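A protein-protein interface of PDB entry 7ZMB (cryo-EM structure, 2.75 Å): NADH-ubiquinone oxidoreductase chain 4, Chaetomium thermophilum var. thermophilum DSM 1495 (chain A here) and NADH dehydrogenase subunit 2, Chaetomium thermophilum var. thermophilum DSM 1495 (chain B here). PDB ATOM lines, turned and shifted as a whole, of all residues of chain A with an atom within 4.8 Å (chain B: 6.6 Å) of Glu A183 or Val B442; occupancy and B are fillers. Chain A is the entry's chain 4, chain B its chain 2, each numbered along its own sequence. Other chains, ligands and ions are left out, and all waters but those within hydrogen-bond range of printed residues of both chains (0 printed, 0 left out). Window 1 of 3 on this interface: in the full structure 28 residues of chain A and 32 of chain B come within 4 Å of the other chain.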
ATOM      1  N   TYR A 179     -23.662   8.784 -15.774  1.00  0.00           N
ATOM      2  CA  TYR A 179     -24.033   7.381 -15.853  1.00  0.00           C
ATOM      3  C   TYR A 179     -24.303   6.942 -17.288  1.00  0.00           C
ATOM      4  O   TYR A 179     -24.035   5.794 -17.645  1.00  0.00           O
ATOM      5  CB  TYR A 179     -25.258   7.133 -14.978  1.00  0.00           C
ATOM      6  CG  TYR A 179     -25.727   5.704 -14.959  1.00  0.00           C
ATOM      7  CD1 TYR A 179     -26.634   5.240 -15.888  1.00  0.00           C
ATOM      8  CD2 TYR A 179     -25.256   4.818 -14.010  1.00  0.00           C
ATOM      9  CE1 TYR A 179     -27.051   3.935 -15.875  1.00  0.00           C
ATOM     10  CE2 TYR A 179     -25.675   3.520 -13.989  1.00  0.00           C
ATOM     11  CZ  TYR A 179     -26.572   3.083 -14.921  1.00  0.00           C
ATOM     12  OH  TYR A 179     -26.995   1.782 -14.904  1.00  0.00           O
ATOM     13  N   ILE A 180     -24.846   7.830 -18.118  1.00  0.00           N
ATOM     14  CA  ILE A 180     -25.161   7.460 -19.491  1.00  0.00           C
ATOM     15  C   ILE A 180     -23.905   7.072 -20.253  1.00  0.00           C
ATOM     16  O   ILE A 180     -23.932   6.167 -21.095  1.00  0.00           O
ATOM     17  CB  ILE A 180     -25.938   8.603 -20.174  1.00  0.00           C
ATOM     18  CG1 ILE A 180     -27.400   8.558 -19.737  1.00  0.00           C
ATOM     19  CG2 ILE A 180     -25.793   8.553 -21.686  1.00  0.00           C
ATOM     20  CD1 ILE A 180     -28.211   9.738 -20.181  1.00  0.00           C
ATOM     21  N   PHE A 181     -22.795   7.725 -19.914  1.00  0.00           N
ATOM     22  CA  PHE A 181     -21.531   7.498 -20.653  1.00  0.00           C
ATOM     23  C   PHE A 181     -20.627   6.500 -19.913  1.00  0.00           C
ATOM     24  O   PHE A 181     -19.825   5.832 -20.584  1.00  0.00           O
ATOM     25  CB  PHE A 181     -20.919   8.858 -20.985  1.00  0.00           C
ATOM     26  CG  PHE A 181     -21.652   9.629 -22.051  1.00  0.00           C
ATOM     27  CD1 PHE A 181     -21.600   9.229 -23.375  1.00  0.00           C
ATOM     28  CD2 PHE A 181     -22.388  10.757 -21.733  1.00  0.00           C
ATOM     29  CE1 PHE A 181     -22.273   9.937 -24.356  1.00  0.00           C
ATOM     30  CE2 PHE A 181     -23.061  11.467 -22.714  1.00  0.00           C
ATOM     31  CZ  PHE A 181     -23.002  11.055 -24.023  1.00  0.00           C
ATOM     32  N   PHE A 182     -20.805   6.259 -18.613  1.00  0.00           N
ATOM     33  CA  PHE A 182     -19.939   5.341 -17.820  1.00  0.00           C
ATOM     34  C   PHE A 182     -20.392   3.900 -18.048  1.00  0.00           C
ATOM     35  O   PHE A 182     -19.647   2.984 -17.704  1.00  0.00           O
ATOM     36  CB  PHE A 182     -19.964   5.790 -16.350  1.00  0.00           C
ATOM     37  CG  PHE A 182     -19.356   4.948 -15.257  1.00  0.00           C
ATOM     38  CD1 PHE A 182     -17.989   4.764 -15.160  1.00  0.00           C
ATOM     39  CD2 PHE A 182     -20.152   4.447 -14.239  1.00  0.00           C
ATOM     40  CE1 PHE A 182     -17.443   4.027 -14.119  1.00  0.00           C
ATOM     41  CE2 PHE A 182     -19.610   3.700 -13.204  1.00  0.00           C
ATOM     42  CZ  PHE A 182     -18.253   3.497 -13.142  1.00  0.00           C
ATOM     43  N   GLU A 183     -21.578   3.714 -18.624  1.00  0.00           N
ATOM     44  CA  GLU A 183     -22.145   2.368 -18.857  1.00  0.00           C
ATOM     45  C   GLU A 183     -22.219   2.149 -20.358  1.00  0.00           C
ATOM     46  O   GLU A 183     -22.459   1.004 -20.772  1.00  0.00           O
ATOM     47  CB  GLU A 183     -23.538   2.239 -18.251  1.00  0.00           C
ATOM     48  CG  GLU A 183     -23.538   1.844 -16.797  1.00  0.00           C
ATOM     49  CD  GLU A 183     -22.601   2.675 -15.947  1.00  0.00           C
ATOM     50  OE1 GLU A 183     -22.852   3.883 -15.806  1.00  0.00           O
ATOM     51  OE2 GLU A 183     -21.600   2.114 -15.466  1.00  0.00           O
ATOM     52  N   SER A 184     -21.996   3.202 -21.136  1.00  0.00           N
ATOM     53  CA  SER A 184     -22.141   3.063 -22.607  1.00  0.00           C
ATOM     54  C   SER A 184     -20.923   2.329 -23.163  1.00  0.00           C
ATOM     55  O   SER A 184     -21.021   1.803 -24.280  1.00  0.00           O
ATOM     56  CB  SER A 184     -22.248   4.411 -23.255  1.00  0.00           C
ATOM     57  OG  SER A 184     -21.012   5.099 -23.179  1.00  0.00           O
ATOM     58  N   ILE A 185     -19.818   2.326 -22.421  1.00  0.00           N
ATOM     59  CA  ILE A 185     -18.601   1.652 -22.858  1.00  0.00           C
ATOM     60  C   ILE A 185     -18.721   0.139 -22.837  1.00  0.00           C
ATOM     61  O   ILE A 185     -17.859  -0.548 -23.385  1.00  0.00           O
ATOM     62  CB  ILE A 185     -17.402   2.089 -21.988  1.00  0.00           C
ATOM     63  CG1 ILE A 185     -17.663   1.762 -20.510  1.00  0.00           C
ATOM     64  CG2 ILE A 185     -17.100   3.565 -22.186  1.00  0.00           C
ATOM     65  CD1 ILE A 185     -16.419   1.558 -19.695  1.00  0.00           C
ATOM     66  N   LEU A 186     -19.764  -0.398 -22.209  1.00  0.00           N
ATOM     67  CA  LEU A 186     -19.886  -1.848 -22.073  1.00  0.00           C
ATOM     68  C   LEU A 186     -20.037  -2.595 -23.391  1.00  0.00           C
ATOM     69  O   LEU A 186     -19.373  -3.632 -23.546  1.00  0.00           O
ATOM     70  CB  LEU A 186     -21.043  -2.191 -21.127  1.00  0.00           C
ATOM     71  CG  LEU A 186     -20.641  -2.445 -19.680  1.00  0.00           C
ATOM     72  CD1 LEU A 186     -19.768  -1.308 -19.220  1.00  0.00           C
ATOM     73  CD2 LEU A 186     -21.865  -2.590 -18.798  1.00  0.00           C
ATOM     74  N   PRO A 187     -20.876  -2.181 -24.339  1.00  0.00           N
ATOM     75  CA  PRO A 187     -21.001  -2.947 -25.582  1.00  0.00           C
ATOM     76  C   PRO A 187     -19.738  -2.908 -26.427  1.00  0.00           C
ATOM     77  O   PRO A 187     -19.306  -3.964 -26.906  1.00  0.00           O
ATOM     78  CB  PRO A 187     -22.191  -2.280 -26.287  1.00  0.00           C
ATOM     79  CG  PRO A 187     -23.008  -1.794 -25.146  1.00  0.00           C
ATOM     80  CD  PRO A 187     -21.992  -1.233 -24.210  1.00  0.00           C
ATOM     81  N   PHE A 209     -18.919  -7.427 -18.439  1.00  0.00           N
ATOM     82  CA  PHE A 209     -20.244  -6.842 -18.753  1.00  0.00           C
ATOM     83  C   PHE A 209     -21.184  -7.033 -17.569  1.00  0.00           C
ATOM     84  O   PHE A 209     -21.904  -6.090 -17.253  1.00  0.00           O
ATOM     85  CB  PHE A 209     -20.812  -7.382 -20.071  1.00  0.00           C
ATOM     86  CG  PHE A 209     -21.955  -6.581 -20.643  1.00  0.00           C
ATOM     87  CD1 PHE A 209     -23.229  -6.669 -20.108  1.00  0.00           C
ATOM     88  CD2 PHE A 209     -21.756  -5.741 -21.725  1.00  0.00           C
ATOM     89  CE1 PHE A 209     -24.276  -5.928 -20.631  1.00  0.00           C
ATOM     90  CE2 PHE A 209     -22.804  -5.002 -22.249  1.00  0.00           C
ATOM     91  CZ  PHE A 209     -24.060  -5.094 -21.701  1.00  0.00           C
ATOM     92  N   THR A 212     -19.961  -4.874 -14.137  1.00  0.00           N
ATOM     93  CA  THR A 212     -20.202  -3.433 -14.386  1.00  0.00           C
ATOM     94  C   THR A 212     -21.698  -3.160 -14.387  1.00  0.00           C
ATOM     95  O   THR A 212     -22.101  -2.213 -13.705  1.00  0.00           O
ATOM     96  CB  THR A 212     -19.591  -2.953 -15.708  1.00  0.00           C
ATOM     97  OG1 THR A 212     -18.233  -3.385 -15.775  1.00  0.00           O
ATOM     98  CG2 THR A 212     -19.650  -1.451 -15.848  1.00  0.00           C
ATOM     99  N   SER A 216     -23.455  -0.766 -11.562  1.00  0.00           N
ATOM    100  CA  SER A 216     -24.024   0.491 -12.092  1.00  0.00           C
ATOM    101  C   SER A 216     -25.505   0.586 -11.753  1.00  0.00           C
ATOM    102  O   SER A 216     -25.965   1.694 -11.531  1.00  0.00           O
ATOM    103  CB  SER A 216     -23.819   0.548 -13.570  1.00  0.00           C
ATOM    104  OG  SER A 216     -24.854  -0.142 -14.252  1.00  0.00           O
ATOM    105  N   ILE B 436     -30.706  -5.760 -29.360  1.00  0.00           N
ATOM    106  CA  ILE B 436     -30.567  -6.616 -28.188  1.00  0.00           C
ATOM    107  C   ILE B 436     -30.014  -5.827 -27.011  1.00  0.00           C
ATOM    108  O   ILE B 436     -30.507  -5.941 -25.886  1.00  0.00           O
ATOM    109  CB  ILE B 436     -29.694  -7.841 -28.516  1.00  0.00           C
ATOM    110  CG1 ILE B 436     -30.440  -8.778 -29.460  1.00  0.00           C
ATOM    111  CG2 ILE B 436     -29.283  -8.566 -27.261  1.00  0.00           C
ATOM    112  CD1 ILE B 436     -31.795  -9.213 -28.924  1.00  0.00           C
ATOM    113  N   PHE B 437     -28.980  -5.017 -27.249  1.00  0.00           N
ATOM    114  CA  PHE B 437     -28.440  -4.187 -26.176  1.00  0.00           C
ATOM    115  C   PHE B 437     -29.486  -3.217 -25.653  1.00  0.00           C
ATOM    116  O   PHE B 437     -29.432  -2.811 -24.490  1.00  0.00           O
ATOM    117  CB  PHE B 437     -27.201  -3.433 -26.663  1.00  0.00           C
ATOM    118  CG  PHE B 437     -25.935  -4.222 -26.563  1.00  0.00           C
ATOM    119  CD1 PHE B 437     -25.588  -4.850 -25.386  1.00  0.00           C
ATOM    120  CD2 PHE B 437     -25.102  -4.360 -27.652  1.00  0.00           C
ATOM    121  CE1 PHE B 437     -24.432  -5.587 -25.298  1.00  0.00           C
ATOM    122  CE2 PHE B 437     -23.945  -5.099 -27.564  1.00  0.00           C
ATOM    123  CZ  PHE B 437     -23.609  -5.708 -26.386  1.00  0.00           C
ATOM    124  N   SER B 438     -30.446  -2.843 -26.498  1.00  0.00           N
ATOM    125  CA  SER B 438     -31.536  -1.983 -26.068  1.00  0.00           C
ATOM    126  C   SER B 438     -32.547  -2.746 -25.222  1.00  0.00           C
ATOM    127  O   SER B 438     -33.182  -2.157 -24.343  1.00  0.00           O
ATOM    128  CB  SER B 438     -32.195  -1.350 -27.291  1.00  0.00           C
ATOM    129  OG  SER B 438     -33.142  -0.365 -26.943  1.00  0.00           O
ATOM    130  N   PHE B 439     -32.718  -4.048 -25.469  1.00  0.00           N
ATOM    131  CA  PHE B 439     -33.515  -4.872 -24.564  1.00  0.00           C
ATOM    132  C   PHE B 439     -32.845  -5.007 -23.209  1.00  0.00           C
ATOM    133  O   PHE B 439     -33.526  -5.079 -22.183  1.00  0.00           O
ATOM    134  CB  PHE B 439     -33.755  -6.264 -25.151  1.00  0.00           C
ATOM    135  CG  PHE B 439     -34.613  -6.277 -26.370  1.00  0.00           C
ATOM    136  CD1 PHE B 439     -35.632  -5.358 -26.530  1.00  0.00           C
ATOM    137  CD2 PHE B 439     -34.396  -7.215 -27.363  1.00  0.00           C
ATOM    138  CE1 PHE B 439     -36.413  -5.375 -27.660  1.00  0.00           C
ATOM    139  CE2 PHE B 439     -35.171  -7.238 -28.493  1.00  0.00           C
ATOM    140  CZ  PHE B 439     -36.184  -6.324 -28.645  1.00  0.00           C
ATOM    141  N   VAL B 440     -31.512  -5.070 -23.181  1.00  0.00           N
ATOM    142  CA  VAL B 440     -30.797  -5.168 -21.912  1.00  0.00           C
ATOM    143  C   VAL B 440     -31.079  -3.945 -21.054  1.00  0.00           C
ATOM    144  O   VAL B 440     -31.455  -4.059 -19.884  1.00  0.00           O
ATOM    145  CB  VAL B 440     -29.285  -5.349 -22.150  1.00  0.00           C
ATOM    146  CG1 VAL B 440     -28.530  -5.291 -20.850  1.00  0.00           C
ATOM    147  CG2 VAL B 440     -29.005  -6.647 -22.837  1.00  0.00           C
ATOM    148  N   GLY B 441     -30.948  -2.774 -21.670  1.00  0.00           N
ATOM    149  CA  GLY B 441     -31.197  -1.528 -20.941  1.00  0.00           C
ATOM    150  C   GLY B 441     -29.922  -0.739 -20.858  1.00  0.00           C
ATOM    151  O   GLY B 441     -29.772   0.006 -19.900  1.00  0.00           O
ATOM    152  N   VAL B 442     -29.047  -0.899 -21.840  1.00  0.00           N
ATOM    153  CA  VAL B 442     -27.725  -0.216 -21.834  1.00  0.00           C
ATOM    154  C   VAL B 442     -27.869   1.209 -22.378  1.00  0.00           C
ATOM    155  O   VAL B 442     -28.476   1.352 -23.442  1.00  0.00           O
ATOM    156  CB  VAL B 442     -26.686  -1.011 -22.656  1.00  0.00           C
ATOM    157  CG1 VAL B 442     -25.276  -0.479 -22.466  1.00  0.00           C
ATOM    158  CG2 VAL B 442     -26.739  -2.494 -22.346  1.00  0.00           C
ATOM    159  N   PRO B 443     -27.311   2.273 -21.745  1.00  0.00           N
ATOM    160  CA  PRO B 443     -27.341   3.610 -22.333  1.00  0.00           C
ATOM    161  C   PRO B 443     -26.331   3.717 -23.462  1.00  0.00           C
ATOM    162  O   PRO B 443     -25.357   2.955 -23.503  1.00  0.00           O
ATOM    163  CB  PRO B 443     -26.981   4.532 -21.157  1.00  0.00           C
ATOM    164  CG  PRO B 443     -26.508   3.664 -20.071  1.00  0.00           C
ATOM    165  CD  PRO B 443     -26.541   2.240 -20.492  1.00  0.00           C
ATOM    166  N   PRO B 444     -26.520   4.655 -24.400  1.00  0.00           N
ATOM    167  CA  PRO B 444     -27.578   5.659 -24.465  1.00  0.00           C
ATOM    168  C   PRO B 444     -28.736   5.249 -25.366  1.00  0.00           C
ATOM    169  O   PRO B 444     -29.355   6.105 -25.989  1.00  0.00           O
ATOM    170  CB  PRO B 444     -26.845   6.864 -25.037  1.00  0.00           C
ATOM    171  CG  PRO B 444     -25.886   6.247 -26.006  1.00  0.00           C
ATOM    172  CD  PRO B 444     -25.547   4.860 -25.485  1.00  0.00           C
ATOM    173  N   LEU B 445     -29.013   3.949 -25.432  1.00  0.00           N
ATOM    174  CA  LEU B 445     -30.070   3.433 -26.281  1.00  0.00           C
ATOM    175  C   LEU B 445     -31.432   3.666 -25.639  1.00  0.00           C
ATOM    176  O   LEU B 445     -31.549   3.929 -24.442  1.00  0.00           O
ATOM    177  CB  LEU B 445     -29.859   1.948 -26.562  1.00  0.00           C
ATOM    178  CG  LEU B 445     -28.475   1.592 -27.095  1.00  0.00           C
ATOM    179  CD1 LEU B 445     -28.326   0.088 -27.236  1.00  0.00           C
ATOM    180  CD2 LEU B 445     -28.195   2.301 -28.401  1.00  0.00           C
ATOM    181  N   VAL B 446     -32.474   3.554 -26.461  1.00  0.00           N
ATOM    182  CA  VAL B 446     -33.813   3.923 -26.021  1.00  0.00           C
ATOM    183  C   VAL B 446     -34.324   2.984 -24.931  1.00  0.00           C
ATOM    184  O   VAL B 446     -35.070   3.406 -24.043  1.00  0.00           O
ATOM    185  CB  VAL B 446     -34.758   3.988 -27.240  1.00  0.00           C
ATOM    186  CG1 VAL B 446     -34.994   2.610 -27.847  1.00  0.00           C
ATOM    187  CG2 VAL B 446     -36.049   4.679 -26.886  1.00  0.00           C
ATOM    188  N   GLY B 447     -33.934   1.710 -24.965  1.00  0.00           N
ATOM    189  CA  GLY B 447     -34.409   0.771 -23.964  1.00  0.00           C
ATOM    190  C   GLY B 447     -33.896   1.055 -22.569  1.00  0.00           C
ATOM    191  O   GLY B 447     -34.573   0.752 -21.585  1.00  0.00           O
ATOM    192  N   PHE B 448     -32.689   1.612 -22.458  1.00  0.00           N
ATOM    193  CA  PHE B 448     -32.199   2.062 -21.160  1.00  0.00           C
ATOM    194  C   PHE B 448     -33.112   3.124 -20.579  1.00  0.00           C
ATOM    195  O   PHE B 448     -33.484   3.072 -19.405  1.00  0.00           O
ATOM    196  CB  PHE B 448     -30.785   2.622 -21.289  1.00  0.00           C
ATOM    197  CG  PHE B 448     -30.403   3.531 -20.164  1.00  0.00           C
ATOM    198  CD1 PHE B 448     -30.091   3.018 -18.922  1.00  0.00           C
ATOM    199  CD2 PHE B 448     -30.389   4.910 -20.335  1.00  0.00           C
ATOM    200  CE1 PHE B 448     -29.767   3.853 -17.883  1.00  0.00           C
ATOM    201  CE2 PHE B 448     -30.059   5.743 -19.292  1.00  0.00           C
ATOM    202  CZ  PHE B 448     -29.745   5.212 -18.070  1.00  0.00           C
ATOM    203  N   PHE B 449     -33.473   4.106 -21.398  1.00  0.00           N
ATOM    204  CA  PHE B 449     -34.287   5.216 -20.929  1.00  0.00           C
ATOM    205  C   PHE B 449     -35.658   4.742 -20.501  1.00  0.00           C
ATOM    206  O   PHE B 449     -36.205   5.223 -19.505  1.00  0.00           O
ATOM    207  CB  PHE B 449     -34.392   6.265 -22.026  1.00  0.00           C
ATOM    208  CG  PHE B 449     -33.154   7.067 -22.193  1.00  0.00           C
ATOM    209  CD1 PHE B 449     -32.812   8.024 -21.264  1.00  0.00           C
ATOM    210  CD2 PHE B 449     -32.315   6.850 -23.265  1.00  0.00           C
ATOM    211  CE1 PHE B 449     -31.669   8.756 -21.415  1.00  0.00           C
ATOM    212  CE2 PHE B 449     -31.173   7.583 -23.413  1.00  0.00           C
ATOM    213  CZ  PHE B 449     -30.851   8.536 -22.491  1.00  0.00           C
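The backbone NH (N) of Val B442 lies within hydrogen-bond range of the backbone carbonyl oxygen (O) of Phe B437, at 3.3 Å. The side-chain hydroxyl (OH) of Tyr A179 sits at hydrogen-bond distance from the side-chain hydroxyl (OG) of Ser A216, at 3.0 Å. The side-chain hydroxyl (OG) of Ser A184 lies within hydrogen-bond range of the backbone carbonyl oxygen (O) of Phe A181, 2.9 Å away.
Ile A180 touches Pro B443. Pro B444 touches Ile A180. Phe B448 touches Ile A180. Phe B449 touches Ile A180. Glu A183 touches Val B442 (O to CG1, 3.6 Å). Ser A184 touches Pro B443. Pro A187 touches Phe B437. Pro A187 touches Val B442. Phe A209 touches Phe B437 (CE2 to CE1, 3.5 Å). Phe A209 touches Val B442.
Of chain B, only Val B442 (3.6 Å) and Pro B443 (3.7 Å) come within 4 Å of Glu A183. Printed residues of chain B within 4 Å of Ser A184: Pro B443. Of the printed residues of chain A, Phe B437 touches Pro A187 (3.6 Å) and Phe A209 (3.5 Å). Phe B439 touches none of the printed residues of chain A. Val B442 touches three residues of chain A. Printed residues of chain A within 4 Å of Pro B444: Ile A180. Of the printed residues of chain A, Phe B449 touches Ile A180 (3.7 Å). The nearest residue of chain B that does not touch Glu A183 is Pro B444 (6.4 Å). The nearest printed residue of chain A that does not touch Val B442 is Ser A184 (4.7 Å). The nearest printed residue of chain B that does not touch Tyr A179 is Pro B443 (4.1 Å).
Of the 12 printed residues of chain A, 6 touch a printed residue of chain B. Printed residues of chain A that touch a printed residue of chain B: Tyr A179, Ile A180, Glu A183, Ser A184, Pro A187 and Phe A209. Hydrophobic or aromatic side chains of chain A within 4 Å of the printed part of chain B: Tyr A179, Ile A180, Pro A187 and Phe A209. Among the printed residues, 12 pairs touch across the chains. Among the printed residues, no Asp or Glu carboxylate lies within 4 Å of a Lys or Arg side-chain nitrogen of the other chain.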
